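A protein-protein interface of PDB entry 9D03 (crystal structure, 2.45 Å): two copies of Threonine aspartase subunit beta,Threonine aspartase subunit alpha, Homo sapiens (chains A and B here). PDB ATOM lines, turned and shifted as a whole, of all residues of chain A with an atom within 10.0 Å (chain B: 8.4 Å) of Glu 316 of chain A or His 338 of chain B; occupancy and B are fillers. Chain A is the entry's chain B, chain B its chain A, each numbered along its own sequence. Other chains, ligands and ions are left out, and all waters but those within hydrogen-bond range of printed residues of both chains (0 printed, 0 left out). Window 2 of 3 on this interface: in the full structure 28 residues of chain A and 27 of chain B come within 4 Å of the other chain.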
ATOM      1  N   GLY A  29      33.033 -28.711  15.533  1.00  0.00           N
ATOM      2  CA  GLY A  29      32.067 -28.926  14.482  1.00  0.00           C
ATOM      3  C   GLY A  29      31.563 -30.346  14.342  1.00  0.00           C
ATOM      4  O   GLY A  29      30.764 -30.601  13.441  1.00  0.00           O
ATOM      5  N   VAL A  31      29.181 -33.192  14.865  1.00  0.00           N
ATOM      6  CA  VAL A  31      27.770 -33.338  15.209  1.00  0.00           C
ATOM      7  C   VAL A  31      27.490 -34.829  15.330  1.00  0.00           C
ATOM      8  O   VAL A  31      27.858 -35.607  14.438  1.00  0.00           O
ATOM      9  CB  VAL A  31      26.866 -32.696  14.132  1.00  0.00           C
ATOM     10  CG1 VAL A  31      25.438 -33.016  14.367  1.00  0.00           C
ATOM     11  CG2 VAL A  31      27.034 -31.198  14.090  1.00  0.00           C
ATOM     12  N   ILE A 261      32.220 -25.608  24.340  1.00  0.00           N
ATOM     13  CA  ILE A 261      30.995 -26.397  24.454  1.00  0.00           C
ATOM     14  C   ILE A 261      30.230 -26.322  23.133  1.00  0.00           C
ATOM     15  O   ILE A 261      29.971 -25.234  22.604  1.00  0.00           O
ATOM     16  CB  ILE A 261      30.138 -25.926  25.643  1.00  0.00           C
ATOM     17  CG1 ILE A 261      30.752 -26.471  26.920  1.00  0.00           C
ATOM     18  CG2 ILE A 261      28.692 -26.400  25.504  1.00  0.00           C
ATOM     19  CD1 ILE A 261      29.992 -26.181  28.160  1.00  0.00           C
ATOM     20  N   GLU A 262      29.855 -27.479  22.609  1.00  0.00           N
ATOM     21  CA  GLU A 262      29.102 -27.566  21.359  1.00  0.00           C
ATOM     22  C   GLU A 262      28.038 -28.618  21.552  1.00  0.00           C
ATOM     23  O   GLU A 262      28.353 -29.806  21.677  1.00  0.00           O
ATOM     24  CB  GLU A 262      29.998 -27.930  20.178  1.00  0.00           C
ATOM     25  CG  GLU A 262      30.825 -26.780  19.653  1.00  0.00           C
ATOM     26  CD  GLU A 262      31.720 -27.172  18.492  1.00  0.00           C
ATOM     27  OE1 GLU A 262      32.359 -28.246  18.559  1.00  0.00           O
ATOM     28  OE2 GLU A 262      31.771 -26.400  17.511  1.00  0.00           O
ATOM     29  N   CYS A 263      26.784 -28.199  21.505  1.00  0.00           N
ATOM     30  CA  CYS A 263      25.667 -29.057  21.858  1.00  0.00           C
ATOM     31  C   CYS A 263      24.855 -29.485  20.641  1.00  0.00           C
ATOM     32  O   CYS A 263      24.642 -28.700  19.709  1.00  0.00           O
ATOM     33  CB  CYS A 263      24.761 -28.321  22.831  1.00  0.00           C
ATOM     34  SG  CYS A 263      25.550 -28.012  24.374  1.00  0.00           S
ATOM     35  N   VAL A 278      19.226 -28.895  16.499  1.00  0.00           N
ATOM     36  CA  VAL A 278      20.428 -28.071  16.482  1.00  0.00           C
ATOM     37  C   VAL A 278      21.659 -28.949  16.655  1.00  0.00           C
ATOM     38  O   VAL A 278      21.640 -29.979  17.341  1.00  0.00           O
ATOM     39  CB  VAL A 278      20.427 -26.955  17.546  1.00  0.00           C
ATOM     40  CG1 VAL A 278      19.344 -25.957  17.223  1.00  0.00           C
ATOM     41  CG2 VAL A 278      20.318 -27.533  18.999  1.00  0.00           C
ATOM     42  N   GLY A 279      22.727 -28.527  16.005  1.00  0.00           N
ATOM     43  CA  GLY A 279      24.000 -29.209  16.104  1.00  0.00           C
ATOM     44  C   GLY A 279      25.112 -28.197  16.278  1.00  0.00           C
ATOM     45  O   GLY A 279      25.016 -27.048  15.831  1.00  0.00           O
ATOM     46  N   ALA A 280      26.176 -28.644  16.931  1.00  0.00           N
ATOM     47  CA  ALA A 280      27.358 -27.822  17.193  1.00  0.00           C
ATOM     48  C   ALA A 280      26.958 -26.435  17.681  1.00  0.00           C
ATOM     49  O   ALA A 280      27.461 -25.409  17.211  1.00  0.00           O
ATOM     50  CB  ALA A 280      28.244 -27.737  15.952  1.00  0.00           C
ATOM     51  N   LEU A 281      26.019 -26.408  18.626  1.00  0.00           N
ATOM     52  CA  LEU A 281      25.490 -25.149  19.128  1.00  0.00           C
ATOM     53  C   LEU A 281      26.256 -24.692  20.367  1.00  0.00           C
ATOM     54  O   LEU A 281      26.386 -25.442  21.345  1.00  0.00           O
ATOM     55  CB  LEU A 281      24.009 -25.292  19.445  1.00  0.00           C
ATOM     56  CG  LEU A 281      23.407 -24.047  20.057  1.00  0.00           C
ATOM     57  CD1 LEU A 281      23.414 -22.943  19.037  1.00  0.00           C
ATOM     58  CD2 LEU A 281      21.994 -24.364  20.471  1.00  0.00           C
ATOM     59  N   SER A 282      26.741 -23.451  20.321  1.00  0.00           N
ATOM     60  CA  SER A 282      27.529 -22.849  21.384  1.00  0.00           C
ATOM     61  C   SER A 282      26.861 -21.581  21.875  1.00  0.00           C
ATOM     62  O   SER A 282      26.242 -20.853  21.103  1.00  0.00           O
ATOM     63  CB  SER A 282      28.932 -22.492  20.890  1.00  0.00           C
ATOM     64  OG  SER A 282      29.702 -23.663  20.719  1.00  0.00           O
ATOM     65  N   GLY A 283      27.020 -21.301  23.158  1.00  0.00           N
ATOM     66  CA  GLY A 283      26.572 -20.040  23.704  1.00  0.00           C
ATOM     67  C   GLY A 283      25.116 -19.979  24.098  1.00  0.00           C
ATOM     68  O   GLY A 283      24.659 -18.914  24.533  1.00  0.00           O
ATOM     69  N   ILE A 284      24.371 -21.075  23.968  1.00  0.00           N
ATOM     70  CA  ILE A 284      22.950 -21.110  24.298  1.00  0.00           C
ATOM     71  C   ILE A 284      22.748 -22.017  25.509  1.00  0.00           C
ATOM     72  O   ILE A 284      23.254 -23.142  25.538  1.00  0.00           O
ATOM     73  CB  ILE A 284      22.126 -21.575  23.086  1.00  0.00           C
ATOM     74  CG1 ILE A 284      22.360 -20.612  21.926  1.00  0.00           C
ATOM     75  CG2 ILE A 284      20.660 -21.647  23.438  1.00  0.00           C
ATOM     76  CD1 ILE A 284      22.025 -19.167  22.266  1.00  0.00           C
ATOM     77  N   VAL A 290      15.954 -24.354  21.601  1.00  0.00           N
ATOM     78  CA  VAL A 290      16.073 -23.920  20.211  1.00  0.00           C
ATOM     79  C   VAL A 290      15.390 -24.926  19.292  1.00  0.00           C
ATOM     80  O   VAL A 290      14.564 -24.561  18.449  1.00  0.00           O
ATOM     81  CB  VAL A 290      17.548 -23.716  19.820  1.00  0.00           C
ATOM     82  CG1 VAL A 290      17.622 -23.091  18.462  1.00  0.00           C
ATOM     83  CG2 VAL A 290      18.271 -22.840  20.867  1.00  0.00           C
ATOM     84  N   LEU A 313      19.354 -26.499  12.308  1.00  0.00           N
ATOM     85  CA  LEU A 313      20.341 -25.426  12.249  1.00  0.00           C
ATOM     86  C   LEU A 313      21.570 -25.812  13.066  1.00  0.00           C
ATOM     87  O   LEU A 313      21.459 -26.490  14.093  1.00  0.00           O
ATOM     88  CB  LEU A 313      19.784 -24.111  12.786  1.00  0.00           C
ATOM     89  CG  LEU A 313      18.594 -23.467  12.091  1.00  0.00           C
ATOM     90  CD1 LEU A 313      18.304 -22.164  12.826  1.00  0.00           C
ATOM     91  CD2 LEU A 313      18.859 -23.204  10.620  1.00  0.00           C
ATOM     92  N   VAL A 314      22.746 -25.375  12.604  1.00  0.00           N
ATOM     93  CA  VAL A 314      24.007 -25.718  13.251  1.00  0.00           C
ATOM     94  C   VAL A 314      24.863 -24.473  13.435  1.00  0.00           C
ATOM     95  O   VAL A 314      24.704 -23.472  12.740  1.00  0.00           O
ATOM     96  CB  VAL A 314      24.803 -26.782  12.456  1.00  0.00           C
ATOM     97  CG1 VAL A 314      23.958 -28.033  12.221  1.00  0.00           C
ATOM     98  CG2 VAL A 314      25.331 -26.200  11.146  1.00  0.00           C
ATOM     99  N   GLY A 315      25.773 -24.547  14.411  1.00  0.00           N
ATOM    100  CA  GLY A 315      26.895 -23.635  14.592  1.00  0.00           C
ATOM    101  C   GLY A 315      26.461 -22.194  14.777  1.00  0.00           C
ATOM    102  O   GLY A 315      25.427 -21.896  15.391  1.00  0.00           O
ATOM    103  N   GLU A 316      27.274 -21.280  14.227  1.00  0.00           N
ATOM    104  CA  GLU A 316      27.049 -19.844  14.414  1.00  0.00           C
ATOM    105  C   GLU A 316      25.648 -19.433  13.978  1.00  0.00           C
ATOM    106  O   GLU A 316      24.979 -18.657  14.668  1.00  0.00           O
ATOM    107  CB  GLU A 316      28.092 -19.042  13.637  1.00  0.00           C
ATOM    108  CG  GLU A 316      29.139 -18.374  14.497  1.00  0.00           C
ATOM    109  CD  GLU A 316      28.525 -17.465  15.534  1.00  0.00           C
ATOM    110  OE1 GLU A 316      28.754 -17.706  16.736  1.00  0.00           O
ATOM    111  OE2 GLU A 316      27.805 -16.519  15.149  1.00  0.00           O
ATOM    112  N   GLY A 317      25.192 -19.936  12.817  1.00  0.00           N
ATOM    113  CA  GLY A 317      23.872 -19.565  12.333  1.00  0.00           C
ATOM    114  C   GLY A 317      22.754 -20.004  13.266  1.00  0.00           C
ATOM    115  O   GLY A 317      21.762 -19.288  13.427  1.00  0.00           O
ATOM    116  N   ALA A 318      22.891 -21.185  13.895  1.00  0.00           N
ATOM    117  CA  ALA A 318      21.911 -21.582  14.905  1.00  0.00           C
ATOM    118  C   ALA A 318      21.922 -20.628  16.097  1.00  0.00           C
ATOM    119  O   ALA A 318      20.859 -20.225  16.592  1.00  0.00           O
ATOM    120  CB  ALA A 318      22.173 -23.009  15.392  1.00  0.00           C
ATOM    121  N   TYR A 319      23.120 -20.249  16.567  1.00  0.00           N
ATOM    122  CA  TYR A 319      23.218 -19.289  17.665  1.00  0.00           C
ATOM    123  C   TYR A 319      22.524 -17.982  17.301  1.00  0.00           C
ATOM    124  O   TYR A 319      21.745 -17.439  18.093  1.00  0.00           O
ATOM    125  CB  TYR A 319      24.690 -19.041  18.023  1.00  0.00           C
ATOM    126  CG  TYR A 319      24.905 -17.913  19.018  1.00  0.00           C
ATOM    127  CD1 TYR A 319      24.665 -18.092  20.372  1.00  0.00           C
ATOM    128  CD2 TYR A 319      25.336 -16.665  18.596  1.00  0.00           C
ATOM    129  CE1 TYR A 319      24.845 -17.069  21.270  1.00  0.00           C
ATOM    130  CE2 TYR A 319      25.526 -15.639  19.487  1.00  0.00           C
ATOM    131  CZ  TYR A 319      25.276 -15.841  20.827  1.00  0.00           C
ATOM    132  OH  TYR A 319      25.461 -14.810  21.716  1.00  0.00           O
ATOM    133  N   ARG A 320      22.793 -17.459  16.100  1.00  0.00           N
ATOM    134  CA  ARG A 320      22.179 -16.197  15.691  1.00  0.00           C
ATOM    135  C   ARG A 320      20.662 -16.322  15.600  1.00  0.00           C
ATOM    136  O   ARG A 320      19.931 -15.428  16.036  1.00  0.00           O
ATOM    137  CB  ARG A 320      22.768 -15.723  14.363  1.00  0.00           C
ATOM    138  N   TRP A 321      20.169 -17.429  15.038  1.00  0.00           N
ATOM    139  CA  TRP A 321      18.727 -17.644  14.971  1.00  0.00           C
ATOM    140  C   TRP A 321      18.119 -17.690  16.365  1.00  0.00           C
ATOM    141  O   TRP A 321      17.060 -17.097  16.608  1.00  0.00           O
ATOM    142  CB  TRP A 321      18.423 -18.939  14.207  1.00  0.00           C
ATOM    143  CG  TRP A 321      16.976 -19.146  13.812  1.00  0.00           C
ATOM    144  CD1 TRP A 321      16.383 -18.771  12.628  1.00  0.00           C
ATOM    145  CD2 TRP A 321      15.954 -19.806  14.573  1.00  0.00           C
ATOM    146  NE1 TRP A 321      15.056 -19.148  12.617  1.00  0.00           N
ATOM    147  CE2 TRP A 321      14.767 -19.783  13.795  1.00  0.00           C
ATOM    148  CE3 TRP A 321      15.919 -20.404  15.838  1.00  0.00           C
ATOM    149  CZ2 TRP A 321      13.563 -20.324  14.246  1.00  0.00           C
ATOM    150  CZ3 TRP A 321      14.728 -20.954  16.280  1.00  0.00           C
ATOM    151  CH2 TRP A 321      13.563 -20.907  15.482  1.00  0.00           C
ATOM    152  N   ALA A 322      18.767 -18.407  17.288  1.00  0.00           N
ATOM    153  CA  ALA A 322      18.262 -18.510  18.657  1.00  0.00           C
ATOM    154  C   ALA A 322      18.240 -17.152  19.344  1.00  0.00           C
ATOM    155  O   ALA A 322      17.262 -16.797  20.010  1.00  0.00           O
ATOM    156  CB  ALA A 322      19.120 -19.482  19.476  1.00  0.00           C
ATOM    157  N   VAL A 323      19.333 -16.395  19.227  1.00  0.00           N
ATOM    158  CA  VAL A 323      19.370 -15.070  19.828  1.00  0.00           C
ATOM    159  C   VAL A 323      18.275 -14.201  19.238  1.00  0.00           C
ATOM    160  O   VAL A 323      17.575 -13.485  19.964  1.00  0.00           O
ATOM    161  CB  VAL A 323      20.763 -14.432  19.669  1.00  0.00           C
ATOM    162  CG1 VAL A 323      20.699 -12.953  20.001  1.00  0.00           C
ATOM    163  CG2 VAL A 323      21.745 -15.107  20.613  1.00  0.00           C
ATOM    164  N   ASP A 324      18.090 -14.267  17.915  1.00  0.00           N
ATOM    165  CA  ASP A 324      17.043 -13.479  17.278  1.00  0.00           C
ATOM    166  C   ASP A 324      15.646 -13.934  17.664  1.00  0.00           C
ATOM    167  O   ASP A 324      14.689 -13.203  17.407  1.00  0.00           O
ATOM    168  CB  ASP A 324      17.169 -13.521  15.754  1.00  0.00           C
ATOM    169  CG  ASP A 324      18.413 -12.841  15.248  1.00  0.00           C
ATOM    170  OD1 ASP A 324      19.098 -12.156  16.043  1.00  0.00           O
ATOM    171  OD2 ASP A 324      18.710 -12.995  14.040  1.00  0.00           O
ATOM    172  N   HIS B  27      18.382 -19.635   5.808  1.00  0.00           N
ATOM    173  CA  HIS B  27      19.033 -19.028   6.961  1.00  0.00           C
ATOM    174  C   HIS B  27      20.423 -19.629   7.138  1.00  0.00           C
ATOM    175  O   HIS B  27      20.627 -20.807   6.840  1.00  0.00           O
ATOM    176  CB  HIS B  27      18.214 -19.238   8.245  1.00  0.00           C
ATOM    177  CG  HIS B  27      18.737 -18.472   9.423  1.00  0.00           C
ATOM    178  ND1 HIS B  27      19.865 -18.857  10.124  1.00  0.00           N
ATOM    179  CD2 HIS B  27      18.295 -17.336  10.018  1.00  0.00           C
ATOM    180  CE1 HIS B  27      20.092 -17.993  11.097  1.00  0.00           C
ATOM    181  NE2 HIS B  27      19.154 -17.060  11.056  1.00  0.00           N
ATOM    182  N   PRO B  28      21.401 -18.846   7.588  1.00  0.00           N
ATOM    183  CA  PRO B  28      22.725 -19.417   7.863  1.00  0.00           C
ATOM    184  C   PRO B  28      22.643 -20.574   8.853  1.00  0.00           C
ATOM    185  O   PRO B  28      21.918 -20.515   9.850  1.00  0.00           O
ATOM    186  CB  PRO B  28      23.507 -18.234   8.437  1.00  0.00           C
ATOM    187  CG  PRO B  28      22.837 -17.026   7.828  1.00  0.00           C
ATOM    188  CD  PRO B  28      21.392 -17.370   7.688  1.00  0.00           C
ATOM    189  N   GLY B  29      23.417 -21.632   8.565  1.00  0.00           N
ATOM    190  CA  GLY B  29      23.443 -22.838   9.356  1.00  0.00           C
ATOM    191  C   GLY B  29      22.364 -23.863   9.042  1.00  0.00           C
ATOM    192  O   GLY B  29      22.333 -24.915   9.692  1.00  0.00           O
ATOM    193  N   ARG B  30      21.475 -23.605   8.094  1.00  0.00           N
ATOM    194  CA  ARG B  30      20.491 -24.623   7.739  1.00  0.00           C
ATOM    195  C   ARG B  30      21.191 -25.768   7.026  1.00  0.00           C
ATOM    196  O   ARG B  30      21.897 -25.551   6.037  1.00  0.00           O
ATOM    197  CB  ARG B  30      19.387 -24.054   6.849  1.00  0.00           C
ATOM    198  CG  ARG B  30      18.227 -25.006   6.653  1.00  0.00           C
ATOM    199  CD  ARG B  30      17.347 -24.579   5.491  1.00  0.00           C
ATOM    200  NE  ARG B  30      16.246 -25.517   5.261  1.00  0.00           N
ATOM    201  CZ  ARG B  30      14.964 -25.169   5.288  1.00  0.00           C
ATOM    202  NH1 ARG B  30      14.618 -23.909   5.512  1.00  0.00           N
ATOM    203  NH2 ARG B  30      14.024 -26.075   5.087  1.00  0.00           N
ATOM    204  N   GLU B 262      26.833 -21.939   1.609  1.00  0.00           N
ATOM    205  CA  GLU B 262      26.930 -22.955   2.651  1.00  0.00           C
ATOM    206  C   GLU B 262      26.545 -24.293   2.044  1.00  0.00           C
ATOM    207  O   GLU B 262      25.385 -24.471   1.656  1.00  0.00           O
ATOM    208  CB  GLU B 262      26.018 -22.658   3.840  1.00  0.00           C
ATOM    209  CG  GLU B 262      26.514 -21.584   4.781  1.00  0.00           C
ATOM    210  CD  GLU B 262      25.568 -21.399   5.942  1.00  0.00           C
ATOM    211  OE1 GLU B 262      26.057 -21.288   7.077  1.00  0.00           O
ATOM    212  OE2 GLU B 262      24.336 -21.395   5.719  1.00  0.00           O
ATOM    213  N   ALA B 280      26.721 -27.148   6.168  1.00  0.00           N
ATOM    214  CA  ALA B 280      26.923 -25.719   6.320  1.00  0.00           C
ATOM    215  C   ALA B 280      28.407 -25.356   6.211  1.00  0.00           C
ATOM    216  O   ALA B 280      28.956 -24.624   7.035  1.00  0.00           O
ATOM    217  CB  ALA B 280      26.309 -25.235   7.634  1.00  0.00           C
ATOM    218  N   VAL B 314      30.511 -29.883  10.698  1.00  0.00           N
ATOM    219  CA  VAL B 314      29.748 -28.759  10.166  1.00  0.00           C
ATOM    220  C   VAL B 314      30.466 -27.430  10.389  1.00  0.00           C
ATOM    221  O   VAL B 314      31.277 -27.272  11.308  1.00  0.00           O
ATOM    222  CB  VAL B 314      28.334 -28.696  10.783  1.00  0.00           C
ATOM    223  CG1 VAL B 314      27.564 -30.013  10.541  1.00  0.00           C
ATOM    224  CG2 VAL B 314      28.414 -28.367  12.285  1.00  0.00           C
ATOM    225  N   GLY B 315      30.140 -26.463   9.531  1.00  0.00           N
ATOM    226  CA  GLY B 315      30.468 -25.064   9.787  1.00  0.00           C
ATOM    227  C   GLY B 315      31.959 -24.832   9.942  1.00  0.00           C
ATOM    228  O   GLY B 315      32.792 -25.453   9.271  1.00  0.00           O
ATOM    229  N   GLU B 316      32.295 -23.946  10.879  1.00  0.00           N
ATOM    230  CA  GLU B 316      33.672 -23.509  11.061  1.00  0.00           C
ATOM    231  C   GLU B 316      34.625 -24.682  11.261  1.00  0.00           C
ATOM    232  O   GLU B 316      35.685 -24.748  10.627  1.00  0.00           O
ATOM    233  CB  GLU B 316      33.737 -22.554  12.255  1.00  0.00           C
ATOM    234  CG  GLU B 316      35.110 -21.964  12.513  1.00  0.00           C
ATOM    235  CD  GLU B 316      35.616 -21.177  11.324  1.00  0.00           C
ATOM    236  OE1 GLU B 316      34.812 -20.435  10.720  1.00  0.00           O
ATOM    237  OE2 GLU B 316      36.812 -21.315  10.988  1.00  0.00           O
ATOM    238  N   HIS B 335      33.356 -17.601   5.750  1.00  0.00           N
ATOM    239  CA  HIS B 335      32.838 -16.633   6.711  1.00  0.00           C
ATOM    240  C   HIS B 335      32.833 -17.221   8.118  1.00  0.00           C
ATOM    241  O   HIS B 335      32.409 -18.365   8.325  1.00  0.00           O
ATOM    242  CB  HIS B 335      31.424 -16.149   6.322  1.00  0.00           C
ATOM    243  CG  HIS B 335      30.500 -17.236   5.854  1.00  0.00           C
ATOM    244  ND1 HIS B 335      29.731 -17.990   6.717  1.00  0.00           N
ATOM    245  CD2 HIS B 335      30.197 -17.671   4.607  1.00  0.00           C
ATOM    246  CE1 HIS B 335      29.006 -18.851   6.026  1.00  0.00           C
ATOM    247  NE2 HIS B 335      29.271 -18.677   4.743  1.00  0.00           N
ATOM    248  N   HIS B 336      33.313 -16.434   9.080  1.00  0.00           N
ATOM    249  CA  HIS B 336      33.330 -16.805  10.494  1.00  0.00           C
ATOM    250  C   HIS B 336      32.678 -15.653  11.252  1.00  0.00           C
ATOM    251  O   HIS B 336      33.374 -14.756  11.735  1.00  0.00           O
ATOM    252  CB  HIS B 336      34.750 -17.075  10.980  1.00  0.00           C
ATOM    253  N   HIS B 337      31.346 -15.688  11.349  1.00  0.00           N
ATOM    254  CA  HIS B 337      30.605 -14.592  11.969  1.00  0.00           C
ATOM    255  C   HIS B 337      31.000 -14.413  13.434  1.00  0.00           C
ATOM    256  O   HIS B 337      31.414 -13.322  13.846  1.00  0.00           O
ATOM    257  CB  HIS B 337      29.101 -14.837  11.823  1.00  0.00           C
ATOM    258  N   HIS B 338      30.877 -15.478  14.231  1.00  0.00           N
ATOM    259  CA  HIS B 338      31.333 -15.548  15.633  1.00  0.00           C
ATOM    260  C   HIS B 338      31.438 -14.213  16.393  1.00  0.00           C
ATOM    261  O   HIS B 338      30.447 -13.685  16.903  1.00  0.00           O
ATOM    262  CB  HIS B 338      32.694 -16.249  15.686  1.00  0.00           C
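Hydrophobic or aromatic side chains of chain A that line the printed part of chain B: Val 31, Ala 280, Leu 313, Val 314 and Trp 321. Of the 13 printed residues of chain B, 8 touch a printed residue of chain A. Hydrophobic or aromatic side chains of chain B that line the printed part of chain A: His 27, Ala 280, Val 314 and His 337. Among the printed residues, 13 pairs touch across the chains.
Glu 316 of chain A touches just these residues of chain B: His 337 (3.9 Å) and His 338 (3.3 Å). Printed residues of chain A within 4 Å of His 338 of chain B: Glu 316. No residue of chain B comes within 4 Å of Gly 315 of chain A. His 336 of chain B touches none of the printed residues of chain A. Of the printed residues of chain B, Trp 321 of chain A touches His 27. Of the printed residues of chain A, Gly 29 of chain B touches Leu 313 and Val 314. The nearest residue of chain B that does not touch Glu 316 of chain A is His 336 of chain B (5.5 Å). The nearest residue of chain A that does not touch His 338 of chain B is Tyr 319 of chain A (5.9 Å). The nearest printed residue of chain A that does not touch His 27 of chain B is Leu 313 of chain A (4.5 Å).
N of Val 314 of chain A is in hydrogen-bond range of O of Gly 29 of chain B. The backbone NH (N) of Val 314 of chain B is in hydrogen-bond range of the backbone carbonyl oxygen (O) of Gly 29 of chain A (2.8 Å). N of His 338 of chain B sits close to OE2 of Glu 316 of chain A (3.4 Å).
The backbone NH (N) of Gly 29 of chain B is in hydrogen-bond range of the side-chain carboxylate (OE2) of Glu 262 of chain B (3.0 Å). The backbone NH (N) of Gly 315 of chain B lies close to the backbone carbonyl oxygen (O) of Ala 280 of chain B. OE1 of Glu 262 of chain A lies within hydrogen-bond range of N of Gly 29 of chain A, at 3.1 Å. O of Cys 263 of chain A sits at hydrogen-bond distance from N of Ala 280 of chain A (3.2 Å). The backbone NH (N) of Gly 279 of chain A sits at hydrogen-bond distance from the backbone carbonyl oxygen (O) of Leu 313 of chain A (3.1 Å). O of Ala 280 of chain A sits close to N of Gly 315 of chain A (3.4 Å).
Gly 29 of chain A touches Val 314 of chain B, and with the chains exchanged Val 314 of chain A touches Gly 29 of chain B. Ala 280 of chain A touches Val 314 of chain B, and with the chains exchanged Val 314 of chain A touches Ala 280 of chain B. Val 314 of chain B touches its own counterpart, Val 314 of chain A. Positions printed for both chains: 29, 262, 280, 314, 315 and 316.
Among the printed residues, merely in contact across the chains: Gly 317 of chain A with His 27 of chain B, Leu 313 of chain A with Gly 29 of chain B, Gly 317 of chain A with Pro 28 of chain B, Trp 321 of chain A with His 27 of chain B, Leu 313 of chain A with Arg 30 of chain B, Val 31 of chain A with Val 314 of chain B, Ala 280 of chain A with Val 314 of chain B, Val 314 of chain A with Ala 280 of chain B, Val 314 of chain A with Val 314 of chain B and Glu 316 of chain A with His 337 of chain B.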
